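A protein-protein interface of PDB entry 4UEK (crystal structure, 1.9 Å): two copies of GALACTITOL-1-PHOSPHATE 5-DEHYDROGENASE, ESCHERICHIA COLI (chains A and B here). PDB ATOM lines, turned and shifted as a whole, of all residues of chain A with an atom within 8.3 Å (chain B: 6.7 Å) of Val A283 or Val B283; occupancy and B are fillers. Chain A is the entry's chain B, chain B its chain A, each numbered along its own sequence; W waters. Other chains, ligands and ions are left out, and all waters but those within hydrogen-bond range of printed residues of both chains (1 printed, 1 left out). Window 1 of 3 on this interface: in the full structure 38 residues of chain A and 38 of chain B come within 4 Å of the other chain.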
ATOM      1  N   ILE A 233      13.236 -21.182  26.921  1.00  0.00           N
ATOM      2  CA  ILE A 233      13.656 -20.035  27.707  1.00  0.00           C
ATOM      3  C   ILE A 233      12.452 -19.192  28.112  1.00  0.00           C
ATOM      4  O   ILE A 233      11.642 -18.787  27.268  1.00  0.00           O
ATOM      5  CB  ILE A 233      14.646 -19.189  26.906  1.00  0.00           C
ATOM      6  CG1 ILE A 233      15.779 -20.085  26.378  1.00  0.00           C
ATOM      7  CG2 ILE A 233      15.162 -18.008  27.740  1.00  0.00           C
ATOM      8  CD1 ILE A 233      16.689 -19.395  25.401  1.00  0.00           C
ATOM      9  N   VAL A 243      15.520  -9.541  27.563  1.00  0.00           N
ATOM     10  CA  VAL A 243      14.971  -9.973  26.274  1.00  0.00           C
ATOM     11  C   VAL A 243      16.091 -10.142  25.251  1.00  0.00           C
ATOM     12  O   VAL A 243      16.155 -11.149  24.536  1.00  0.00           O
ATOM     13  CB  VAL A 243      13.922  -8.983  25.723  1.00  0.00           C
ATOM     14  CG1 VAL A 243      13.523  -9.380  24.321  1.00  0.00           C
ATOM     15  CG2 VAL A 243      12.692  -8.962  26.620  1.00  0.00           C
ATOM     16  N   ALA A 246      18.255 -13.205  26.080  1.00  0.00           N
ATOM     17  CA  ALA A 246      17.650 -14.482  25.715  1.00  0.00           C
ATOM     18  C   ALA A 246      17.953 -14.840  24.268  1.00  0.00           C
ATOM     19  O   ALA A 246      18.289 -15.985  23.953  1.00  0.00           O
ATOM     20  CB  ALA A 246      16.148 -14.454  25.950  1.00  0.00           C
ATOM     21  N   VAL A 247      17.841 -13.860  23.383  1.00  0.00           N
ATOM     22  CA  VAL A 247      18.128 -14.088  21.971  1.00  0.00           C
ATOM     23  C   VAL A 247      19.603 -14.422  21.747  1.00  0.00           C
ATOM     24  O   VAL A 247      19.944 -15.354  21.002  1.00  0.00           O
ATOM     25  CB  VAL A 247      17.729 -12.857  21.125  1.00  0.00           C
ATOM     26  CG1 VAL A 247      18.180 -13.036  19.662  1.00  0.00           C
ATOM     27  CG2 VAL A 247      16.226 -12.644  21.204  1.00  0.00           C
ATOM     28  N   HIS A 253      17.034 -23.476  17.191  1.00  0.00           N
ATOM     29  CA  HIS A 253      15.602 -23.761  17.276  1.00  0.00           C
ATOM     30  C   HIS A 253      15.016 -23.702  18.687  1.00  0.00           C
ATOM     31  O   HIS A 253      14.023 -24.367  18.966  1.00  0.00           O
ATOM     32  CB  HIS A 253      15.304 -25.127  16.658  1.00  0.00           C
ATOM     33  CG  HIS A 253      15.477 -25.154  15.169  1.00  0.00           C
ATOM     34  ND1 HIS A 253      14.415 -25.282  14.303  1.00  0.00           N
ATOM     35  CD2 HIS A 253      16.581 -25.039  14.400  1.00  0.00           C
ATOM     36  CE1 HIS A 253      14.860 -25.258  13.056  1.00  0.00           C
ATOM     37  NE2 HIS A 253      16.171 -25.110  13.086  1.00  0.00           N
ATOM     38  N   ALA A 254      15.603 -22.872  19.546  1.00  0.00           N
ATOM     39  CA  ALA A 254      15.127 -22.721  20.916  1.00  0.00           C
ATOM     40  C   ALA A 254      13.750 -22.076  20.903  1.00  0.00           C
ATOM     41  O   ALA A 254      13.436 -21.282  20.007  1.00  0.00           O
ATOM     42  CB  ALA A 254      16.101 -21.884  21.739  1.00  0.00           C
ATOM     43  N   GLN A 255      12.925 -22.449  21.873  1.00  0.00           N
ATOM     44  CA  GLN A 255      11.669 -21.761  22.134  1.00  0.00           C
ATOM     45  C   GLN A 255      11.923 -20.676  23.163  1.00  0.00           C
ATOM     46  O   GLN A 255      12.538 -20.929  24.195  1.00  0.00           O
ATOM     47  CB  GLN A 255      10.606 -22.712  22.655  1.00  0.00           C
ATOM     48  CG  GLN A 255      10.076 -23.721  21.679  1.00  0.00           C
ATOM     49  CD  GLN A 255       9.279 -24.780  22.390  1.00  0.00           C
ATOM     50  OE1 GLN A 255       9.830 -25.552  23.179  1.00  0.00           O
ATOM     51  NE2 GLN A 255       7.973 -24.816  22.142  1.00  0.00           N
ATOM     52  N   LEU A 256      11.434 -19.480  22.887  1.00  0.00           N
ATOM     53  CA  LEU A 256      11.638 -18.341  23.772  1.00  0.00           C
ATOM     54  C   LEU A 256      10.290 -17.765  24.190  1.00  0.00           C
ATOM     55  O   LEU A 256       9.611 -17.130  23.394  1.00  0.00           O
ATOM     56  CB  LEU A 256      12.497 -17.285  23.079  1.00  0.00           C
ATOM     57  CG  LEU A 256      12.831 -15.979  23.788  1.00  0.00           C
ATOM     58  CD1 LEU A 256      13.166 -16.244  25.237  1.00  0.00           C
ATOM     59  CD2 LEU A 256      14.000 -15.306  23.082  1.00  0.00           C
ATOM     60  N   ALA A 257       9.910 -18.008  25.440  1.00  0.00           N
ATOM     61  CA  ALA A 257       8.594 -17.605  25.948  1.00  0.00           C
ATOM     62  C   ALA A 257       8.680 -16.292  26.716  1.00  0.00           C
ATOM     63  O   ALA A 257       9.453 -16.158  27.669  1.00  0.00           O
ATOM     64  CB  ALA A 257       8.019 -18.697  26.834  1.00  0.00           C
ATOM     65  N   LEU A 258       7.899 -15.312  26.290  1.00  0.00           N
ATOM     66  CA  LEU A 258       7.954 -13.990  26.873  1.00  0.00           C
ATOM     67  C   LEU A 258       6.817 -13.829  27.873  1.00  0.00           C
ATOM     68  O   LEU A 258       5.646 -13.836  27.489  1.00  0.00           O
ATOM     69  CB  LEU A 258       7.868 -12.916  25.778  1.00  0.00           C
ATOM     70  CG  LEU A 258       8.984 -12.933  24.720  1.00  0.00           C
ATOM     71  CD1 LEU A 258       8.780 -11.804  23.704  1.00  0.00           C
ATOM     72  CD2 LEU A 258      10.382 -12.863  25.363  1.00  0.00           C
ATOM     73  N   PHE A 273      18.624  -9.098  16.119  1.00  0.00           N
ATOM     74  CA  PHE A 273      17.404  -9.473  15.410  1.00  0.00           C
ATOM     75  C   PHE A 273      17.696 -10.619  14.452  1.00  0.00           C
ATOM     76  O   PHE A 273      16.921 -11.563  14.336  1.00  0.00           O
ATOM     77  CB  PHE A 273      16.832  -8.277  14.634  1.00  0.00           C
ATOM     78  CG  PHE A 273      15.629  -8.618  13.796  1.00  0.00           C
ATOM     79  CD1 PHE A 273      14.363  -8.602  14.344  1.00  0.00           C
ATOM     80  CD2 PHE A 273      15.768  -8.951  12.459  1.00  0.00           C
ATOM     81  CE1 PHE A 273      13.243  -8.918  13.576  1.00  0.00           C
ATOM     82  CE2 PHE A 273      14.660  -9.262  11.683  1.00  0.00           C
ATOM     83  CZ  PHE A 273      13.393  -9.248  12.249  1.00  0.00           C
ATOM     84  N   ILE A 276      17.503 -14.134  15.680  1.00  0.00           N
ATOM     85  CA  ILE A 276      16.162 -14.718  15.726  1.00  0.00           C
ATOM     86  C   ILE A 276      15.920 -15.498  14.442  1.00  0.00           C
ATOM     87  O   ILE A 276      15.390 -16.613  14.473  1.00  0.00           O
ATOM     88  CB  ILE A 276      15.051 -13.650  15.908  1.00  0.00           C
ATOM     89  CG1 ILE A 276      15.256 -12.887  17.208  1.00  0.00           C
ATOM     90  CG2 ILE A 276      13.675 -14.303  15.908  1.00  0.00           C
ATOM     91  CD1 ILE A 276      14.419 -11.627  17.304  1.00  0.00           C
ATOM     92  N   LEU A 277      16.340 -14.925  13.313  1.00  0.00           N
ATOM     93  CA  LEU A 277      16.216 -15.614  12.038  1.00  0.00           C
ATOM     94  C   LEU A 277      17.212 -16.761  11.936  1.00  0.00           C
ATOM     95  O   LEU A 277      16.833 -17.888  11.635  1.00  0.00           O
ATOM     96  CB  LEU A 277      16.420 -14.646  10.863  1.00  0.00           C
ATOM     97  CG  LEU A 277      15.168 -13.880  10.422  1.00  0.00           C
ATOM     98  CD1 LEU A 277      14.652 -13.008  11.535  1.00  0.00           C
ATOM     99  CD2 LEU A 277      15.444 -13.060   9.169  1.00  0.00           C
ATOM    100  N   GLU A 280      16.657 -19.706  13.864  1.00  0.00           N
ATOM    101  CA  GLU A 280      15.272 -20.114  13.658  1.00  0.00           C
ATOM    102  C   GLU A 280      14.567 -20.328  15.007  1.00  0.00           C
ATOM    103  O   GLU A 280      14.029 -21.394  15.287  1.00  0.00           O
ATOM    104  CB  GLU A 280      15.205 -21.355  12.771  1.00  0.00           C
ATOM    105  CG  GLU A 280      15.579 -21.015  11.323  1.00  0.00           C
ATOM    106  CD  GLU A 280      15.346 -22.157  10.344  1.00  0.00           C
ATOM    107  OE1 GLU A 280      15.562 -23.325  10.712  1.00  0.00           O
ATOM    108  OE2 GLU A 280      14.948 -21.888   9.193  1.00  0.00           O
ATOM    109  N   LEU A 281      14.599 -19.290  15.837  1.00  0.00           N
ATOM    110  CA  LEU A 281      13.926 -19.306  17.133  1.00  0.00           C
ATOM    111  C   LEU A 281      12.409 -19.257  16.971  1.00  0.00           C
ATOM    112  O   LEU A 281      11.879 -18.817  15.941  1.00  0.00           O
ATOM    113  CB  LEU A 281      14.393 -18.123  17.997  1.00  0.00           C
ATOM    114  CG  LEU A 281      15.899 -18.034  18.266  1.00  0.00           C
ATOM    115  CD1 LEU A 281      16.242 -16.833  19.129  1.00  0.00           C
ATOM    116  CD2 LEU A 281      16.418 -19.331  18.918  1.00  0.00           C
ATOM    117  N   THR A 282      11.714 -19.721  17.994  1.00  0.00           N
ATOM    118  CA  THR A 282      10.276 -19.531  18.068  1.00  0.00           C
ATOM    119  C   THR A 282      10.004 -18.672  19.287  1.00  0.00           C
ATOM    120  O   THR A 282      10.252 -19.093  20.407  1.00  0.00           O
ATOM    121  CB  THR A 282       9.521 -20.855  18.166  1.00  0.00           C
ATOM    122  OG1 THR A 282       9.734 -21.599  16.965  1.00  0.00           O
ATOM    123  CG2 THR A 282       8.017 -20.596  18.314  1.00  0.00           C
ATOM    124  N   VAL A 283       9.536 -17.451  19.059  1.00  0.00           N
ATOM    125  CA  VAL A 283       9.254 -16.532  20.151  1.00  0.00           C
ATOM    126  C   VAL A 283       7.757 -16.563  20.458  1.00  0.00           C
ATOM    127  O   VAL A 283       6.929 -16.285  19.596  1.00  0.00           O
ATOM    128  CB  VAL A 283       9.717 -15.113  19.822  1.00  0.00           C
ATOM    129  CG1 VAL A 283       9.430 -14.181  21.001  1.00  0.00           C
ATOM    130  CG2 VAL A 283      11.213 -15.122  19.518  1.00  0.00           C
ATOM    131  N   ILE A 284       7.432 -16.924  21.698  1.00  0.00           N
ATOM    132  CA  ILE A 284       6.058 -17.213  22.096  1.00  0.00           C
ATOM    133  C   ILE A 284       5.568 -16.156  23.067  1.00  0.00           C
ATOM    134  O   ILE A 284       6.023 -16.091  24.210  1.00  0.00           O
ATOM    135  CB  ILE A 284       5.958 -18.618  22.756  1.00  0.00           C
ATOM    136  CG1 ILE A 284       6.445 -19.697  21.783  1.00  0.00           C
ATOM    137  CG2 ILE A 284       4.549 -18.919  23.215  1.00  0.00           C
ATOM    138  CD1 ILE A 284       6.669 -21.049  22.439  1.00  0.00           C
ATOM    139  N   GLY A 285       4.667 -15.303  22.605  1.00  0.00           N
ATOM    140  CA  GLY A 285       4.069 -14.320  23.487  1.00  0.00           C
ATOM    141  C   GLY A 285       3.174 -15.045  24.475  1.00  0.00           C
ATOM    142  O   GLY A 285       2.388 -15.930  24.089  1.00  0.00           O
ATOM    143  N   SER A 286       3.282 -14.677  25.746  1.00  0.00           N
ATOM    144  CA  SER A 286       2.470 -15.308  26.766  1.00  0.00           C
ATOM    145  C   SER A 286       1.739 -14.254  27.570  1.00  0.00           C
ATOM    146  O   SER A 286       2.362 -13.311  28.064  1.00  0.00           O
ATOM    147  CB  SER A 286       3.325 -16.170  27.698  1.00  0.00           C
ATOM    148  OG  SER A 286       2.496 -16.875  28.608  1.00  0.00           O
ATOM    149  N   VAL B 247       3.440  -6.752  13.787  1.00  0.00           N
ATOM    150  CA  VAL B 247       2.968  -6.882  15.166  1.00  0.00           C
ATOM    151  C   VAL B 247       1.709  -6.048  15.432  1.00  0.00           C
ATOM    152  O   VAL B 247       0.752  -6.511  16.062  1.00  0.00           O
ATOM    153  CB  VAL B 247       4.082  -6.475  16.167  1.00  0.00           C
ATOM    154  CG1 VAL B 247       3.529  -6.361  17.572  1.00  0.00           C
ATOM    155  CG2 VAL B 247       5.234  -7.490  16.120  1.00  0.00           C
ATOM    156  N   ALA B 254      -1.963 -14.996  16.113  1.00  0.00           N
ATOM    157  CA  ALA B 254      -1.389 -15.044  14.783  1.00  0.00           C
ATOM    158  C   ALA B 254       0.046 -15.588  14.808  1.00  0.00           C
ATOM    159  O   ALA B 254       0.804 -15.355  15.754  1.00  0.00           O
ATOM    160  CB  ALA B 254      -1.420 -13.668  14.141  1.00  0.00           C
ATOM    161  N   GLN B 255       0.395 -16.347  13.774  1.00  0.00           N
ATOM    162  CA  GLN B 255       1.781 -16.694  13.506  1.00  0.00           C
ATOM    163  C   GLN B 255       2.444 -15.623  12.659  1.00  0.00           C
ATOM    164  O   GLN B 255       1.903 -15.202  11.638  1.00  0.00           O
ATOM    165  CB  GLN B 255       1.898 -18.027  12.788  1.00  0.00           C
ATOM    166  CG  GLN B 255       1.331 -19.200  13.540  1.00  0.00           C
ATOM    167  CD  GLN B 255       1.110 -20.368  12.612  1.00  0.00           C
ATOM    168  OE1 GLN B 255       0.235 -20.326  11.743  1.00  0.00           O
ATOM    169  NE2 GLN B 255       1.918 -21.418  12.774  1.00  0.00           N
ATOM    170  N   LEU B 256       3.630 -15.208  13.082  1.00  0.00           N
ATOM    171  CA  LEU B 256       4.399 -14.196  12.385  1.00  0.00           C
ATOM    172  C   LEU B 256       5.746 -14.787  11.949  1.00  0.00           C
ATOM    173  O   LEU B 256       6.605 -15.039  12.786  1.00  0.00           O
ATOM    174  CB  LEU B 256       4.592 -12.984  13.288  1.00  0.00           C
ATOM    175  CG  LEU B 256       5.292 -11.734  12.776  1.00  0.00           C
ATOM    176  CD1 LEU B 256       4.812 -11.427  11.385  1.00  0.00           C
ATOM    177  CD2 LEU B 256       5.006 -10.564  13.712  1.00  0.00           C
ATOM    178  N   ALA B 257       5.899 -15.041  10.649  1.00  0.00           N
ATOM    179  CA  ALA B 257       7.118 -15.633  10.104  1.00  0.00           C
ATOM    180  C   ALA B 257       8.051 -14.549   9.578  1.00  0.00           C
ATOM    181  O   ALA B 257       7.645 -13.706   8.783  1.00  0.00           O
ATOM    182  CB  ALA B 257       6.780 -16.630   9.009  1.00  0.00           C
ATOM    183  N   LEU B 258       9.286 -14.538  10.068  1.00  0.00           N
ATOM    184  CA  LEU B 258      10.230 -13.484   9.733  1.00  0.00           C
ATOM    185  C   LEU B 258      11.204 -14.040   8.705  1.00  0.00           C
ATOM    186  O   LEU B 258      11.992 -14.934   9.010  1.00  0.00           O
ATOM    187  CB  LEU B 258      10.980 -12.978  10.970  1.00  0.00           C
ATOM    188  CG  LEU B 258      10.126 -12.410  12.114  1.00  0.00           C
ATOM    189  CD1 LEU B 258      11.000 -11.993  13.284  1.00  0.00           C
ATOM    190  CD2 LEU B 258       9.317 -11.228  11.611  1.00  0.00           C
ATOM    191  N   ILE B 276       2.974  -8.260  21.358  1.00  0.00           N
ATOM    192  CA  ILE B 276       3.450  -9.625  21.125  1.00  0.00           C
ATOM    193  C   ILE B 276       2.945 -10.541  22.234  1.00  0.00           C
ATOM    194  O   ILE B 276       2.434 -11.619  21.964  1.00  0.00           O
ATOM    195  CB  ILE B 276       4.987  -9.710  21.056  1.00  0.00           C
ATOM    196  CG1 ILE B 276       5.519  -8.883  19.881  1.00  0.00           C
ATOM    197  CG2 ILE B 276       5.411 -11.154  20.945  1.00  0.00           C
ATOM    198  CD1 ILE B 276       7.016  -8.629  19.963  1.00  0.00           C
ATOM    199  N   LEU B 281       1.232 -13.831  20.293  1.00  0.00           N
ATOM    200  CA  LEU B 281       1.731 -14.132  18.958  1.00  0.00           C
ATOM    201  C   LEU B 281       2.788 -15.209  19.052  1.00  0.00           C
ATOM    202  O   LEU B 281       3.410 -15.437  20.111  1.00  0.00           O
ATOM    203  CB  LEU B 281       2.314 -12.895  18.276  1.00  0.00           C
ATOM    204  CG  LEU B 281       1.372 -11.699  18.092  1.00  0.00           C
ATOM    205  CD1 LEU B 281       2.087 -10.603  17.316  1.00  0.00           C
ATOM    206  CD2 LEU B 281       0.053 -12.106  17.393  1.00  0.00           C
ATOM    207  N   THR B 282       2.983 -15.878  17.932  1.00  0.00           N
ATOM    208  CA  THR B 282       4.100 -16.787  17.800  1.00  0.00           C
ATOM    209  C   THR B 282       4.979 -16.213  16.695  1.00  0.00           C
ATOM    210  O   THR B 282       4.556 -16.117  15.549  1.00  0.00           O
ATOM    211  CB  THR B 282       3.633 -18.200  17.491  1.00  0.00           C
ATOM    212  OG1 THR B 282       2.873 -18.686  18.608  1.00  0.00           O
ATOM    213  CG2 THR B 282       4.820 -19.118  17.271  1.00  0.00           C
ATOM    214  N   VAL B 283       6.177 -15.769  17.057  1.00  0.00           N
ATOM    215  CA  VAL B 283       7.070 -15.202  16.069  1.00  0.00           C
ATOM    216  C   VAL B 283       8.070 -16.271  15.646  1.00  0.00           C
ATOM    217  O   VAL B 283       8.817 -16.810  16.479  1.00  0.00           O
ATOM    218  CB  VAL B 283       7.801 -13.960  16.592  1.00  0.00           C
ATOM    219  CG1 VAL B 283       8.724 -13.393  15.496  1.00  0.00           C
ATOM    220  CG2 VAL B 283       6.805 -12.915  17.060  1.00  0.00           C
ATOM    221  N   ILE B 284       8.074 -16.574  14.351  1.00  0.00           N
ATOM    222  CA  ILE B 284       8.862 -17.677  13.807  1.00  0.00           C
ATOM    223  C   ILE B 284      10.026 -17.186  12.946  1.00  0.00           C
ATOM    224  O   ILE B 284       9.820 -16.673  11.848  1.00  0.00           O
ATOM    225  CB  ILE B 284       7.970 -18.620  12.957  1.00  0.00           C
ATOM    226  CG1 ILE B 284       6.798 -19.150  13.785  1.00  0.00           C
ATOM    227  CG2 ILE B 284       8.769 -19.776  12.397  1.00  0.00           C
ATOM    228  CD1 ILE B 284       5.671 -19.724  12.920  1.00  0.00           C
ATOM    229  N   GLY B 285      11.244 -17.341  13.448  1.00  0.00           N
ATOM    230  CA  GLY B 285      12.429 -16.999  12.683  1.00  0.00           C
ATOM    231  C   GLY B 285      12.596 -17.989  11.543  1.00  0.00           C
ATOM    232  O   GLY B 285      12.541 -19.206  11.747  1.00  0.00           O
HETATM  233  O   HOH W   1       2.033 -17.480  21.843  1.00  0.00           O
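N of Gly A285 is in hydrogen-bond range of O of Leu B281.
The backbone NH (N) of Val B283 lies within hydrogen-bond range of the backbone carbonyl oxygen (O) of Val A283.
N of Gly B285 lies within hydrogen-bond range of O of Leu A281 (3.0 Å).
The backbone carbonyl oxygen (O) of Leu B256 lies within hydrogen-bond range of the backbone NH (N) of Ile B284 (2.6 Å).
The backbone NH (N) of Leu B258 lies within hydrogen-bond range of the backbone carbonyl oxygen (O) of Ile B284.
A ring nitrogen (NE2) of His A253 is in hydrogen-bond range of the side-chain carboxylate (OE1) of Glu A280 (3.0 Å).
O of Ala A254 sits at hydrogen-bond distance from N of Thr A282 (3.1 Å).
The backbone NH of Ile A284 lies within hydrogen-bond range of the backbone carbonyl oxygen of Leu A256 (2.8 Å).
O of Ile A284 lies within hydrogen-bond range of N of Leu A258 (2.9 Å).
Phe A273 touches Leu B258 (CZ to CD1, 3.8 Å).
Glu A280 touches Gly B285 (CA to O, 3.5 Å).
Val B283 touches Leu A281 (O to O, 3.7 Å).
Leu A281 touches Ile B284.
Thr B282 touches Thr A282 (CG2 to CG2, 3.7 Å).
Thr A282 touches Val B283.
Val A283 touches Leu B281 (O to O, 3.7 Å).
CA of Thr B282 touches O of Val A283, 3.4 Å away.
Ile A284 touches Leu B281.
CA of Gly A285 touches O of Ile B276 (3.5 Å).
Of chain B, only Leu B281 (3.7 Å), Thr B282 (3.4 Å) and Val B283 (2.7 Å) come within 4 Å of Val A283.
Of chain A, only Leu A281, Thr A282 and Val A283 come within 4 Å of Val B283.
Of the printed residues of chain B, Thr A282 touches Thr B282 and Val B283.
Of the printed residues of chain B, Gly A285 touches Ile B276 (3.5 Å) and Leu B281 (2.8 Å).
Of the printed residues of chain A, Ile B284 touches Leu A281.
Of the printed residues of chain A, Leu B258 touches Phe A273 (3.8 Å) and Leu A277 (3.6 Å).
Val A247 touches none of the printed residues of chain B.
The nearest residue of chain A that does not touch Val B283 is Ile A284 (4.9 Å).
Of the 12 printed residues of chain B, 7 touch a printed residue of chain A.
Hydrophobic or aromatic side chains of chain B that line the printed part of chain A: Leu B258 and Val B283.
Of the 20 printed residues of chain A, 9 touch a printed residue of chain B.
Ile A276 touches Gly B285, and with the chains exchanged Gly A285 touches Ile B276.
Leu A281 touches Val B283, and with the chains exchanged Val A283 touches Leu B281.
Leu A281 touches Gly B285, and with the chains exchanged Gly A285 touches Leu B281.
Val B283 touches its own counterpart, Val A283.
12 positions are printed for both chains.
Water W1 lies within hydrogen-bond range of O of Gly A285 (2.8 Å) and O of Leu B281 (3.0 Å).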
